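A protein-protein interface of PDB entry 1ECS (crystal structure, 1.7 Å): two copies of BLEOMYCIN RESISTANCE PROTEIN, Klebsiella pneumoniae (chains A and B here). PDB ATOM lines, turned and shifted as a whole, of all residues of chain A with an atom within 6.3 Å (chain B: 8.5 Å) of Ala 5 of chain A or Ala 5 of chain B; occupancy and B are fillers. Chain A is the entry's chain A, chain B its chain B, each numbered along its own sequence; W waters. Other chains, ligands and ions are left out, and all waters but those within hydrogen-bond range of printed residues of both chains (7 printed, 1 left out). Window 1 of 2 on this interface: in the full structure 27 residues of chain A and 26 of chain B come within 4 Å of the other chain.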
ATOM      1  N   ASP A   3      17.770  24.335  26.372  1.00  0.00           N
ATOM      2  CA  ASP A   3      17.264  22.979  26.559  1.00  0.00           C
ATOM      3  C   ASP A   3      16.245  22.597  25.499  1.00  0.00           C
ATOM      4  O   ASP A   3      15.346  23.356  25.147  1.00  0.00           O
ATOM      5  CB  ASP A   3      16.602  22.814  27.922  1.00  0.00           C
ATOM      6  CG  ASP A   3      17.563  23.105  29.061  1.00  0.00           C
ATOM      7  OD1 ASP A   3      17.059  23.649  30.061  1.00  0.00           O
ATOM      8  OD2 ASP A   3      18.773  22.819  28.982  1.00  0.00           O
ATOM      9  N   GLN A   4      16.343  21.367  24.981  1.00  0.00           N
ATOM     10  CA  GLN A   4      15.262  21.017  24.041  1.00  0.00           C
ATOM     11  C   GLN A   4      15.019  19.518  24.054  1.00  0.00           C
ATOM     12  O   GLN A   4      15.917  18.677  24.151  1.00  0.00           O
ATOM     13  CB  GLN A   4      15.620  21.603  22.682  1.00  0.00           C
ATOM     14  CG  GLN A   4      16.141  20.646  21.638  1.00  0.00           C
ATOM     15  CD  GLN A   4      16.238  21.309  20.267  1.00  0.00           C
ATOM     16  OE1 GLN A   4      15.349  22.051  19.845  1.00  0.00           O
ATOM     17  NE2 GLN A   4      17.330  21.044  19.558  1.00  0.00           N
ATOM     18  N   ALA A   5      13.733  19.128  23.990  1.00  0.00           N
ATOM     19  CA  ALA A   5      13.391  17.721  23.888  1.00  0.00           C
ATOM     20  C   ALA A   5      13.089  17.417  22.430  1.00  0.00           C
ATOM     21  O   ALA A   5      12.367  18.180  21.796  1.00  0.00           O
ATOM     22  CB  ALA A   5      12.175  17.380  24.731  1.00  0.00           C
ATOM     23  N   THR A   6      13.613  16.333  21.879  1.00  0.00           N
ATOM     24  CA  THR A   6      13.277  16.112  20.467  1.00  0.00           C
ATOM     25  C   THR A   6      12.664  14.730  20.337  1.00  0.00           C
ATOM     26  O   THR A   6      12.983  13.810  21.075  1.00  0.00           O
ATOM     27  CB  THR A   6      14.524  16.214  19.577  1.00  0.00           C
ATOM     28  OG1 THR A   6      15.439  15.207  20.022  1.00  0.00           O
ATOM     29  CG2 THR A   6      15.227  17.544  19.774  1.00  0.00           C
ATOM     30  N   PRO A   7      11.757  14.573  19.383  1.00  0.00           N
ATOM     31  CA  PRO A   7      11.240  13.252  19.079  1.00  0.00           C
ATOM     32  C   PRO A   7      12.340  12.377  18.476  1.00  0.00           C
ATOM     33  O   PRO A   7      13.297  12.879  17.878  1.00  0.00           O
ATOM     34  CB  PRO A   7      10.194  13.516  18.002  1.00  0.00           C
ATOM     35  CG  PRO A   7      10.108  14.981  17.791  1.00  0.00           C
ATOM     36  CD  PRO A   7      11.208  15.656  18.563  1.00  0.00           C
ATOM     37  N   ASP A  42      13.459  26.079  13.625  1.00  0.00           N
ATOM     38  CA  ASP A  42      13.590  25.608  14.999  1.00  0.00           C
ATOM     39  C   ASP A  42      13.044  24.201  15.178  1.00  0.00           C
ATOM     40  O   ASP A  42      13.044  23.682  16.303  1.00  0.00           O
ATOM     41  CB  ASP A  42      12.838  26.553  15.952  1.00  0.00           C
ATOM     42  CG  ASP A  42      13.571  27.880  16.099  1.00  0.00           C
ATOM     43  OD1 ASP A  42      14.781  27.866  16.394  1.00  0.00           O
ATOM     44  OD2 ASP A  42      12.923  28.929  15.907  1.00  0.00           O
ATOM     45  N   LEU A  43      12.562  23.598  14.084  1.00  0.00           N
ATOM     46  CA  LEU A  43      12.038  22.239  14.223  1.00  0.00           C
ATOM     47  C   LEU A  43      13.200  21.244  14.093  1.00  0.00           C
ATOM     48  O   LEU A  43      13.937  21.343  13.108  1.00  0.00           O
ATOM     49  CB  LEU A  43      10.993  21.933  13.169  1.00  0.00           C
ATOM     50  CG  LEU A  43       9.698  22.740  13.143  1.00  0.00           C
ATOM     51  CD1 LEU A  43       8.989  22.513  11.817  1.00  0.00           C
ATOM     52  CD2 LEU A  43       8.816  22.365  14.326  1.00  0.00           C
ATOM     53  N   MET A  44      13.370  20.333  15.028  1.00  0.00           N
ATOM     54  CA  MET A  44      14.409  19.318  14.984  1.00  0.00           C
ATOM     55  C   MET A  44      13.768  17.948  15.154  1.00  0.00           C
ATOM     56  O   MET A  44      13.055  17.656  16.118  1.00  0.00           O
ATOM     57  CB  MET A  44      15.496  19.534  16.042  1.00  0.00           C
ATOM     58  CG  MET A  44      16.556  18.436  16.010  1.00  0.00           C
ATOM     59  SD  MET A  44      18.085  18.849  16.905  1.00  0.00           S
ATOM     60  CE  MET A  44      18.534  20.306  15.977  1.00  0.00           C
ATOM     61  N   LEU A  45      14.019  17.068  14.177  1.00  0.00           N
ATOM     62  CA  LEU A  45      13.511  15.705  14.253  1.00  0.00           C
ATOM     63  C   LEU A  45      14.685  14.713  14.178  1.00  0.00           C
ATOM     64  O   LEU A  45      15.530  14.884  13.306  1.00  0.00           O
ATOM     65  CB  LEU A  45      12.559  15.339  13.120  1.00  0.00           C
ATOM     66  CG  LEU A  45      11.377  16.247  12.843  1.00  0.00           C
ATOM     67  CD1 LEU A  45      10.633  15.853  11.576  1.00  0.00           C
ATOM     68  CD2 LEU A  45      10.427  16.223  14.042  1.00  0.00           C
ATOM     69  N   CYS A  62       4.513  12.385  16.817  1.00  0.00           N
ATOM     70  CA  CYS A  62       5.106  13.519  17.522  1.00  0.00           C
ATOM     71  C   CYS A  62       4.199  14.719  17.245  1.00  0.00           C
ATOM     72  O   CYS A  62       3.315  14.549  16.399  1.00  0.00           O
ATOM     73  CB  CYS A  62       6.541  13.786  17.087  1.00  0.00           C
ATOM     74  SG  CYS A  62       6.670  14.425  15.394  1.00  0.00           S
ATOM     75  N   CYS A  63       4.397  15.851  17.911  1.00  0.00           N
ATOM     76  CA  CYS A  63       3.659  17.043  17.529  1.00  0.00           C
ATOM     77  C   CYS A  63       4.547  18.077  16.854  1.00  0.00           C
ATOM     78  O   CYS A  63       5.674  18.239  17.305  1.00  0.00           O
ATOM     79  CB  CYS A  63       3.037  17.748  18.758  1.00  0.00           C
ATOM     80  SG  CYS A  63       1.768  16.664  19.469  1.00  0.00           S
ATOM     81  N   LEU A  64       4.013  18.740  15.834  1.00  0.00           N
ATOM     82  CA  LEU A  64       4.628  19.962  15.328  1.00  0.00           C
ATOM     83  C   LEU A  64       3.714  21.141  15.720  1.00  0.00           C
ATOM     84  O   LEU A  64       2.632  21.292  15.181  1.00  0.00           O
ATOM     85  CB  LEU A  64       4.858  19.979  13.821  1.00  0.00           C
ATOM     86  CG  LEU A  64       5.629  18.834  13.174  1.00  0.00           C
ATOM     87  CD1 LEU A  64       6.057  19.228  11.756  1.00  0.00           C
ATOM     88  CD2 LEU A  64       6.837  18.404  13.997  1.00  0.00           C
ATOM     89  N   ARG A  65       4.182  21.935  16.674  1.00  0.00           N
ATOM     90  CA  ARG A  65       3.469  23.117  17.164  1.00  0.00           C
ATOM     91  C   ARG A  65       4.076  24.320  16.443  1.00  0.00           C
ATOM     92  O   ARG A  65       5.195  24.735  16.697  1.00  0.00           O
ATOM     93  CB  ARG A  65       3.545  23.222  18.694  1.00  0.00           C
ATOM     94  CG  ARG A  65       2.794  22.047  19.351  1.00  0.00           C
ATOM     95  CD  ARG A  65       3.009  21.994  20.865  1.00  0.00           C
ATOM     96  NE  ARG A  65       2.222  20.904  21.457  1.00  0.00           N
ATOM     97  CZ  ARG A  65       0.921  21.010  21.732  1.00  0.00           C
ATOM     98  NH1 ARG A  65       0.310  22.163  21.455  1.00  0.00           N
ATOM     99  NH2 ARG A  65       0.231  20.010  22.267  1.00  0.00           N
ATOM    100  N   THR B   2       7.003  30.394  18.287  1.00  0.00           N
ATOM    101  CA  THR B   2       8.186  29.622  17.912  1.00  0.00           C
ATOM    102  C   THR B   2       7.814  28.192  17.549  1.00  0.00           C
ATOM    103  O   THR B   2       7.092  27.541  18.304  1.00  0.00           O
ATOM    104  CB  THR B   2       9.215  29.586  19.054  1.00  0.00           C
ATOM    105  OG1 THR B   2       9.539  30.936  19.418  1.00  0.00           O
ATOM    106  CG2 THR B   2      10.500  28.903  18.609  1.00  0.00           C
ATOM    107  N   ASP B   3       8.293  27.706  16.410  1.00  0.00           N
ATOM    108  CA  ASP B   3       8.014  26.342  15.987  1.00  0.00           C
ATOM    109  C   ASP B   3       8.718  25.339  16.901  1.00  0.00           C
ATOM    110  O   ASP B   3       9.849  25.595  17.295  1.00  0.00           O
ATOM    111  CB  ASP B   3       8.483  26.041  14.573  1.00  0.00           C
ATOM    112  CG  ASP B   3       7.854  26.908  13.509  1.00  0.00           C
ATOM    113  OD1 ASP B   3       8.558  27.083  12.484  1.00  0.00           O
ATOM    114  OD2 ASP B   3       6.709  27.378  13.668  1.00  0.00           O
ATOM    115  N   GLN B   4       8.029  24.240  17.214  1.00  0.00           N
ATOM    116  CA  GLN B   4       8.703  23.245  18.054  1.00  0.00           C
ATOM    117  C   GLN B   4       8.105  21.865  17.828  1.00  0.00           C
ATOM    118  O   GLN B   4       6.912  21.644  17.646  1.00  0.00           O
ATOM    119  CB  GLN B   4       8.663  23.669  19.503  1.00  0.00           C
ATOM    120  CG  GLN B   4       7.355  23.491  20.235  1.00  0.00           C
ATOM    121  CD  GLN B   4       7.591  23.613  21.744  1.00  0.00           C
ATOM    122  OE1 GLN B   4       8.594  23.102  22.260  1.00  0.00           O
ATOM    123  NE2 GLN B   4       6.667  24.288  22.417  1.00  0.00           N
ATOM    124  N   ALA B   5       9.033  20.898  17.815  1.00  0.00           N
ATOM    125  CA  ALA B   5       8.626  19.517  17.619  1.00  0.00           C
ATOM    126  C   ALA B   5       8.701  18.856  18.987  1.00  0.00           C
ATOM    127  O   ALA B   5       9.731  19.024  19.632  1.00  0.00           O
ATOM    128  CB  ALA B   5       9.521  18.784  16.640  1.00  0.00           C
ATOM    129  N   THR B   6       7.637  18.156  19.387  1.00  0.00           N
ATOM    130  CA  THR B   6       7.691  17.543  20.710  1.00  0.00           C
ATOM    131  C   THR B   6       7.474  16.045  20.612  1.00  0.00           C
ATOM    132  O   THR B   6       6.719  15.545  19.789  1.00  0.00           O
ATOM    133  CB  THR B   6       6.624  18.157  21.638  1.00  0.00           C
ATOM    134  OG1 THR B   6       5.348  17.865  21.050  1.00  0.00           O
ATOM    135  CG2 THR B   6       6.718  19.663  21.700  1.00  0.00           C
ATOM    136  N   PRO B   7       8.162  15.322  21.486  1.00  0.00           N
ATOM    137  CA  PRO B   7       8.004  13.899  21.602  1.00  0.00           C
ATOM    138  C   PRO B   7       6.578  13.585  22.094  1.00  0.00           C
ATOM    139  O   PRO B   7       5.996  14.436  22.784  1.00  0.00           O
ATOM    140  CB  PRO B   7       8.979  13.519  22.714  1.00  0.00           C
ATOM    141  CG  PRO B   7       9.799  14.707  23.006  1.00  0.00           C
ATOM    142  CD  PRO B   7       9.139  15.918  22.424  1.00  0.00           C
ATOM    143  N   ASN B   8       6.076  12.430  21.711  1.00  0.00           N
ATOM    144  CA  ASN B   8       4.820  11.879  22.205  1.00  0.00           C
ATOM    145  C   ASN B   8       5.148  10.535  22.829  1.00  0.00           C
ATOM    146  O   ASN B   8       5.564   9.620  22.120  1.00  0.00           O
ATOM    147  CB  ASN B   8       3.779  11.699  21.121  1.00  0.00           C
ATOM    148  CG  ASN B   8       3.252  12.975  20.502  1.00  0.00           C
ATOM    149  OD1 ASN B   8       2.458  12.857  19.583  1.00  0.00           O
ATOM    150  ND2 ASN B   8       3.653  14.145  20.969  1.00  0.00           N
ATOM    151  N   LEU B   9       4.978  10.441  24.131  1.00  0.00           N
ATOM    152  CA  LEU B   9       5.424   9.279  24.886  1.00  0.00           C
ATOM    153  C   LEU B   9       4.279   8.578  25.600  1.00  0.00           C
ATOM    154  O   LEU B   9       3.305   9.226  25.975  1.00  0.00           O
ATOM    155  CB  LEU B   9       6.470   9.719  25.911  1.00  0.00           C
ATOM    156  CG  LEU B   9       7.671  10.472  25.313  1.00  0.00           C
ATOM    157  CD1 LEU B   9       8.517  11.026  26.437  1.00  0.00           C
ATOM    158  CD2 LEU B   9       8.507   9.572  24.401  1.00  0.00           C
ATOM    159  N   PHE B  26       9.533  18.958  36.311  1.00  0.00           N
ATOM    160  CA  PHE B  26       8.465  19.137  35.327  1.00  0.00           C
ATOM    161  C   PHE B  26       7.116  19.481  35.951  1.00  0.00           C
ATOM    162  O   PHE B  26       6.710  18.861  36.942  1.00  0.00           O
ATOM    163  CB  PHE B  26       8.308  17.843  34.516  1.00  0.00           C
ATOM    164  CG  PHE B  26       9.469  17.592  33.553  1.00  0.00           C
ATOM    165  CD1 PHE B  26      10.625  16.981  34.021  1.00  0.00           C
ATOM    166  CD2 PHE B  26       9.355  17.969  32.212  1.00  0.00           C
ATOM    167  CE1 PHE B  26      11.691  16.747  33.147  1.00  0.00           C
ATOM    168  CE2 PHE B  26      10.414  17.739  31.332  1.00  0.00           C
ATOM    169  CZ  PHE B  26      11.564  17.132  31.817  1.00  0.00           C
ATOM    170  N   LEU B  38       3.821  17.869  30.005  1.00  0.00           N
ATOM    171  CA  LEU B  38       4.679  18.284  31.127  1.00  0.00           C
ATOM    172  C   LEU B  38       5.732  19.261  30.618  1.00  0.00           C
ATOM    173  O   LEU B  38       6.178  19.098  29.475  1.00  0.00           O
ATOM    174  CB  LEU B  38       5.401  17.105  31.772  1.00  0.00           C
ATOM    175  CG  LEU B  38       4.526  15.989  32.356  1.00  0.00           C
ATOM    176  CD1 LEU B  38       5.384  14.940  33.068  1.00  0.00           C
ATOM    177  CD2 LEU B  38       3.485  16.563  33.307  1.00  0.00           C
ATOM    178  N   ARG B  40       9.327  21.619  31.722  1.00  0.00           N
ATOM    179  CA  ARG B  40      10.406  22.060  32.591  1.00  0.00           C
ATOM    180  C   ARG B  40      11.216  23.094  31.807  1.00  0.00           C
ATOM    181  O   ARG B  40      12.077  22.715  31.007  1.00  0.00           O
ATOM    182  CB  ARG B  40      11.279  20.895  33.039  1.00  0.00           C
ATOM    183  CG  ARG B  40      12.497  21.327  33.853  1.00  0.00           C
ATOM    184  CD  ARG B  40      13.579  20.264  33.744  1.00  0.00           C
ATOM    185  NE  ARG B  40      14.354  20.080  34.974  1.00  0.00           N
ATOM    186  CZ  ARG B  40      15.611  20.490  35.049  1.00  0.00           C
ATOM    187  NH1 ARG B  40      16.130  21.072  33.976  1.00  0.00           N
ATOM    188  NH2 ARG B  40      16.340  20.335  36.136  1.00  0.00           N
ATOM    189  N   ASP B  42      12.292  25.143  28.905  1.00  0.00           N
ATOM    190  CA  ASP B  42      12.019  24.971  27.479  1.00  0.00           C
ATOM    191  C   ASP B  42      11.830  23.514  27.084  1.00  0.00           C
ATOM    192  O   ASP B  42      11.528  23.252  25.912  1.00  0.00           O
ATOM    193  CB  ASP B  42      13.151  25.576  26.637  1.00  0.00           C
ATOM    194  CG  ASP B  42      13.380  27.037  26.976  1.00  0.00           C
ATOM    195  OD1 ASP B  42      12.388  27.782  27.048  1.00  0.00           O
ATOM    196  OD2 ASP B  42      14.546  27.418  27.192  1.00  0.00           O
ATOM    197  N   LEU B  43      11.999  22.567  28.003  1.00  0.00           N
ATOM    198  CA  LEU B  43      11.736  21.165  27.730  1.00  0.00           C
ATOM    199  C   LEU B  43      10.243  20.847  27.754  1.00  0.00           C
ATOM    200  O   LEU B  43       9.638  21.058  28.812  1.00  0.00           O
ATOM    201  CB  LEU B  43      12.421  20.300  28.792  1.00  0.00           C
ATOM    202  CG  LEU B  43      13.945  20.235  28.806  1.00  0.00           C
ATOM    203  CD1 LEU B  43      14.422  19.338  29.943  1.00  0.00           C
ATOM    204  CD2 LEU B  43      14.502  19.728  27.480  1.00  0.00           C
ATOM    205  N   MET B  44       9.650  20.332  26.694  1.00  0.00           N
ATOM    206  CA  MET B  44       8.234  19.964  26.693  1.00  0.00           C
ATOM    207  C   MET B  44       8.061  18.493  26.312  1.00  0.00           C
ATOM    208  O   MET B  44       8.599  18.084  25.282  1.00  0.00           O
ATOM    209  CB  MET B  44       7.446  20.852  25.719  1.00  0.00           C
ATOM    210  CG  MET B  44       5.937  20.659  25.813  1.00  0.00           C
ATOM    211  SD  MET B  44       4.982  21.836  24.800  1.00  0.00           S
ATOM    212  CE  MET B  44       4.928  23.190  25.976  1.00  0.00           C
ATOM    213  N   LEU B  45       7.339  17.714  27.119  1.00  0.00           N
ATOM    214  CA  LEU B  45       7.025  16.324  26.830  1.00  0.00           C
ATOM    215  C   LEU B  45       5.514  16.116  26.850  1.00  0.00           C
ATOM    216  O   LEU B  45       4.834  16.615  27.750  1.00  0.00           O
ATOM    217  CB  LEU B  45       7.673  15.399  27.852  1.00  0.00           C
ATOM    218  CG  LEU B  45       9.184  15.484  28.070  1.00  0.00           C
ATOM    219  CD1 LEU B  45       9.566  14.578  29.246  1.00  0.00           C
ATOM    220  CD2 LEU B  45       9.933  15.110  26.805  1.00  0.00           C
ATOM    221  N   GLU B  46       4.983  15.407  25.879  1.00  0.00           N
ATOM    222  CA  GLU B  46       3.560  15.097  25.780  1.00  0.00           C
ATOM    223  C   GLU B  46       3.370  13.599  25.906  1.00  0.00           C
ATOM    224  O   GLU B  46       4.134  12.814  25.345  1.00  0.00           O
ATOM    225  CB  GLU B  46       2.980  15.589  24.450  1.00  0.00           C
ATOM    226  CG  GLU B  46       3.505  16.960  24.066  1.00  0.00           C
ATOM    227  CD  GLU B  46       2.603  17.755  23.142  1.00  0.00           C
ATOM    228  OE1 GLU B  46       1.363  17.618  23.120  1.00  0.00           O
ATOM    229  OE2 GLU B  46       3.142  18.577  22.362  1.00  0.00           O
ATOM    230  N   CYS B  62      13.245   9.530  23.415  1.00  0.00           N
ATOM    231  CA  CYS B  62      13.360  10.905  22.924  1.00  0.00           C
ATOM    232  C   CYS B  62      14.747  11.390  23.354  1.00  0.00           C
ATOM    233  O   CYS B  62      15.406  10.662  24.120  1.00  0.00           O
ATOM    234  CB  CYS B  62      12.245  11.817  23.453  1.00  0.00           C
ATOM    235  SG  CYS B  62      12.364  12.016  25.254  1.00  0.00           S
ATOM    236  N   CYS B  63      15.143  12.549  22.872  1.00  0.00           N
ATOM    237  CA  CYS B  63      16.367  13.168  23.384  1.00  0.00           C
ATOM    238  C   CYS B  63      16.067  14.394  24.228  1.00  0.00           C
ATOM    239  O   CYS B  63      15.204  15.161  23.811  1.00  0.00           O
ATOM    240  CB  CYS B  63      17.270  13.659  22.231  1.00  0.00           C
ATOM    241  SG  CYS B  63      17.918  12.230  21.317  1.00  0.00           S
ATOM    242  N   LEU B  64      16.777  14.563  25.336  1.00  0.00           N
ATOM    243  CA  LEU B  64      16.855  15.815  26.065  1.00  0.00           C
ATOM    244  C   LEU B  64      18.271  16.375  25.826  1.00  0.00           C
ATOM    245  O   LEU B  64      19.264  15.852  26.342  1.00  0.00           O
ATOM    246  CB  LEU B  64      16.585  15.666  27.554  1.00  0.00           C
ATOM    247  CG  LEU B  64      15.322  14.916  27.991  1.00  0.00           C
ATOM    248  CD1 LEU B  64      15.170  15.024  29.503  1.00  0.00           C
ATOM    249  CD2 LEU B  64      14.085  15.413  27.253  1.00  0.00           C
ATOM    250  N   ARG B  65      18.288  17.424  25.024  1.00  0.00           N
ATOM    251  CA  ARG B  65      19.517  18.171  24.710  1.00  0.00           C
ATOM    252  C   ARG B  65      19.606  19.344  25.684  1.00  0.00           C
ATOM    253  O   ARG B  65      18.800  20.270  25.573  1.00  0.00           O
ATOM    254  CB  ARG B  65      19.497  18.562  23.226  1.00  0.00           C
ATOM    255  CG  ARG B  65      19.658  17.319  22.328  1.00  0.00           C
ATOM    256  CD  ARG B  65      19.546  17.689  20.831  1.00  0.00           C
ATOM    257  NE  ARG B  65      19.714  16.441  20.063  1.00  0.00           N
ATOM    258  CZ  ARG B  65      20.910  15.937  19.761  1.00  0.00           C
ATOM    259  NH1 ARG B  65      22.010  16.579  20.139  1.00  0.00           N
ATOM    260  NH2 ARG B  65      21.056  14.803  19.081  1.00  0.00           N
ATOM    261  N   LEU B  66      20.532  19.253  26.628  1.00  0.00           N
ATOM    262  CA  LEU B  66      20.642  20.041  27.838  1.00  0.00           C
ATOM    263  C   LEU B  66      21.852  20.957  27.876  1.00  0.00           C
ATOM    264  O   LEU B  66      22.959  20.568  27.471  1.00  0.00           O
ATOM    265  CB  LEU B  66      20.711  19.091  29.062  1.00  0.00           C
ATOM    266  CG  LEU B  66      19.496  18.135  29.144  1.00  0.00           C
ATOM    267  CD1 LEU B  66      19.601  17.083  30.236  1.00  0.00           C
ATOM    268  CD2 LEU B  66      18.223  18.954  29.328  1.00  0.00           C
ATOM    269  N   LEU B 114      15.007   8.118  27.778  1.00  0.00           N
ATOM    270  CA  LEU B 114      15.310   9.523  27.531  1.00  0.00           C
ATOM    271  C   LEU B 114      16.831   9.604  27.428  1.00  0.00           C
ATOM    272  O   LEU B 114      17.521   9.365  28.419  1.00  0.00           O
ATOM    273  CB  LEU B 114      14.698  10.434  28.607  1.00  0.00           C
ATOM    274  CG  LEU B 114      13.141  10.390  28.585  1.00  0.00           C
ATOM    275  CD1 LEU B 114      12.616   9.327  29.536  1.00  0.00           C
ATOM    276  CD2 LEU B 114      12.503  11.718  28.946  1.00  0.00           C
ATOM    277  N   ARG B 115      17.331   9.885  26.220  1.00  0.00           N
ATOM    278  CA  ARG B 115      18.775  10.107  26.066  1.00  0.00           C
ATOM    279  C   ARG B 115      19.103  11.510  26.529  1.00  0.00           C
ATOM    280  O   ARG B 115      18.534  12.483  26.012  1.00  0.00           O
ATOM    281  CB  ARG B 115      19.182   9.896  24.601  1.00  0.00           C
ATOM    282  CG  ARG B 115      18.680   8.568  24.057  1.00  0.00           C
ATOM    283  CD  ARG B 115      18.953   8.364  22.581  1.00  0.00           C
ATOM    284  NE  ARG B 115      17.880   7.611  21.936  1.00  0.00           N
ATOM    285  CZ  ARG B 115      17.927   6.352  21.546  1.00  0.00           C
ATOM    286  NH1 ARG B 115      19.002   5.599  21.700  1.00  0.00           N
ATOM    287  NH2 ARG B 115      16.851   5.826  20.973  1.00  0.00           N
ATOM    288  N   ASN B 119      24.699  19.673  25.434  1.00  0.00           N
ATOM    289  CA  ASN B 119      24.766  20.577  24.302  1.00  0.00           C
ATOM    290  C   ASN B 119      26.219  21.023  24.093  1.00  0.00           C
ATOM    291  O   ASN B 119      26.920  21.289  25.073  1.00  0.00           O
ATOM    292  CB  ASN B 119      23.880  21.805  24.499  1.00  0.00           C
ATOM    293  CG  ASN B 119      22.412  21.474  24.264  1.00  0.00           C
ATOM    294  OD1 ASN B 119      22.120  20.476  23.599  1.00  0.00           O
ATOM    295  ND2 ASN B 119      21.504  22.280  24.798  1.00  0.00           N
HETATM  296  O   HOH W   1      11.098  27.726  12.720  1.00  0.00           O
HETATM  297  O   HOH W   2      14.978  25.309  29.894  1.00  0.00           O
HETATM  298  O   HOH W   3      16.622  26.443  28.069  1.00  0.00           O
HETATM  299  O   HOH W   4      10.208  29.305  15.084  1.00  0.00           O
HETATM  300  O   HOH W   5      14.863  22.386  31.504  1.00  0.00           O
HETATM  301  O   HOH W   6      11.975  21.377  17.540  1.00  0.00           O
HETATM  302  O   HOH W   7      11.544  20.923  24.472  1.00  0.00           O
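Of the 24 printed residues of chain B, 17 touch a printed residue of chain A. Hydrophobic or aromatic side chains of chain B that line the printed part of chain A: Ala 5, Pro 7, Leu 43, Leu 45, Leu 64 and Leu 66.
The backbone NH (N) of Gln 4 of chain A lies within hydrogen-bond range of the backbone carbonyl oxygen (O) of Arg 65 of chain B, 2.8 Å away. O of Cys 63 of chain B is in hydrogen-bond range of N of Thr 6 of chain A (2.8 Å). N of Cys 62 of chain A sits close to OD1 of Asn 8 of chain B (3.5 Å). The backbone carbonyl oxygen of Cys 63 of chain A is in hydrogen-bond range of the backbone NH of Thr 6 of chain B (2.9 Å). SG of Cys 63 of chain A lies within hydrogen-bond range of ND2 of Asn 8 of chain B. The side-chain sulfur (SG) of Cys 63 of chain A sits close to the side-chain carboxylate (OE2) of Glu 46 of chain B (3.7 Å). N of Arg 65 of chain A sits at hydrogen-bond distance from O of Gln 4 of chain B (2.9 Å). The guanidinium group of Arg 65 of chain A lies within salt-bridge range of the side-chain carboxylate of Glu 46 of chain B (2.7 Å).
Gln 4 of chain A touches Leu 43 of chain B, and with the chains exchanged Leu 43 of chain A touches Gln 4 of chain B. Ala 5 of chain A touches Cys 63 of chain B, and with the chains exchanged Cys 63 of chain A touches Ala 5 of chain B.
Ala 5 of chain A touches just these residues of chain B: Ala 5, Pro 7, Leu 43, Met 44, Leu 45, Cys 63 and Leu 64. Ala 5 of chain B touches seven residues of chain A. Of the printed residues of chain A, Asp 3 of chain B touches Asp 42, Leu 43 and Arg 65. Of the printed residues of chain A, Leu 66 of chain B touches Asp 3. Printed residues of chain A within 4 Å of Cys 62 of chain B: Thr 6 (3.2 Å). The nearest residue of chain B that does not touch Ala 5 of chain A is Thr 6 of chain B (4.8 Å). The nearest residue of chain A that does not touch Ala 5 of chain B is Thr 6 of chain A (4.7 Å). The nearest printed residue of chain B that does not touch Gln 4 of chain A is Asp 42 of chain B (4.7 Å).
OE2 of Glu 46 of chain B lies within hydrogen-bond range of OG1 of Thr 6 of chain B, at 2.7 Å. N of Leu 9 of chain B lies within hydrogen-bond range of O of Glu 46 of chain B, at 2.8 Å.
Water W3 bridges OD2 of Asp 42 of chain B (2.5 Å) and N of Asp 3 of chain A (2.9 Å). Water W4 lies within hydrogen-bond range of the backbone NH of Asp 3 of chain B and the side-chain carboxylate of Asp 42 of chain A.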
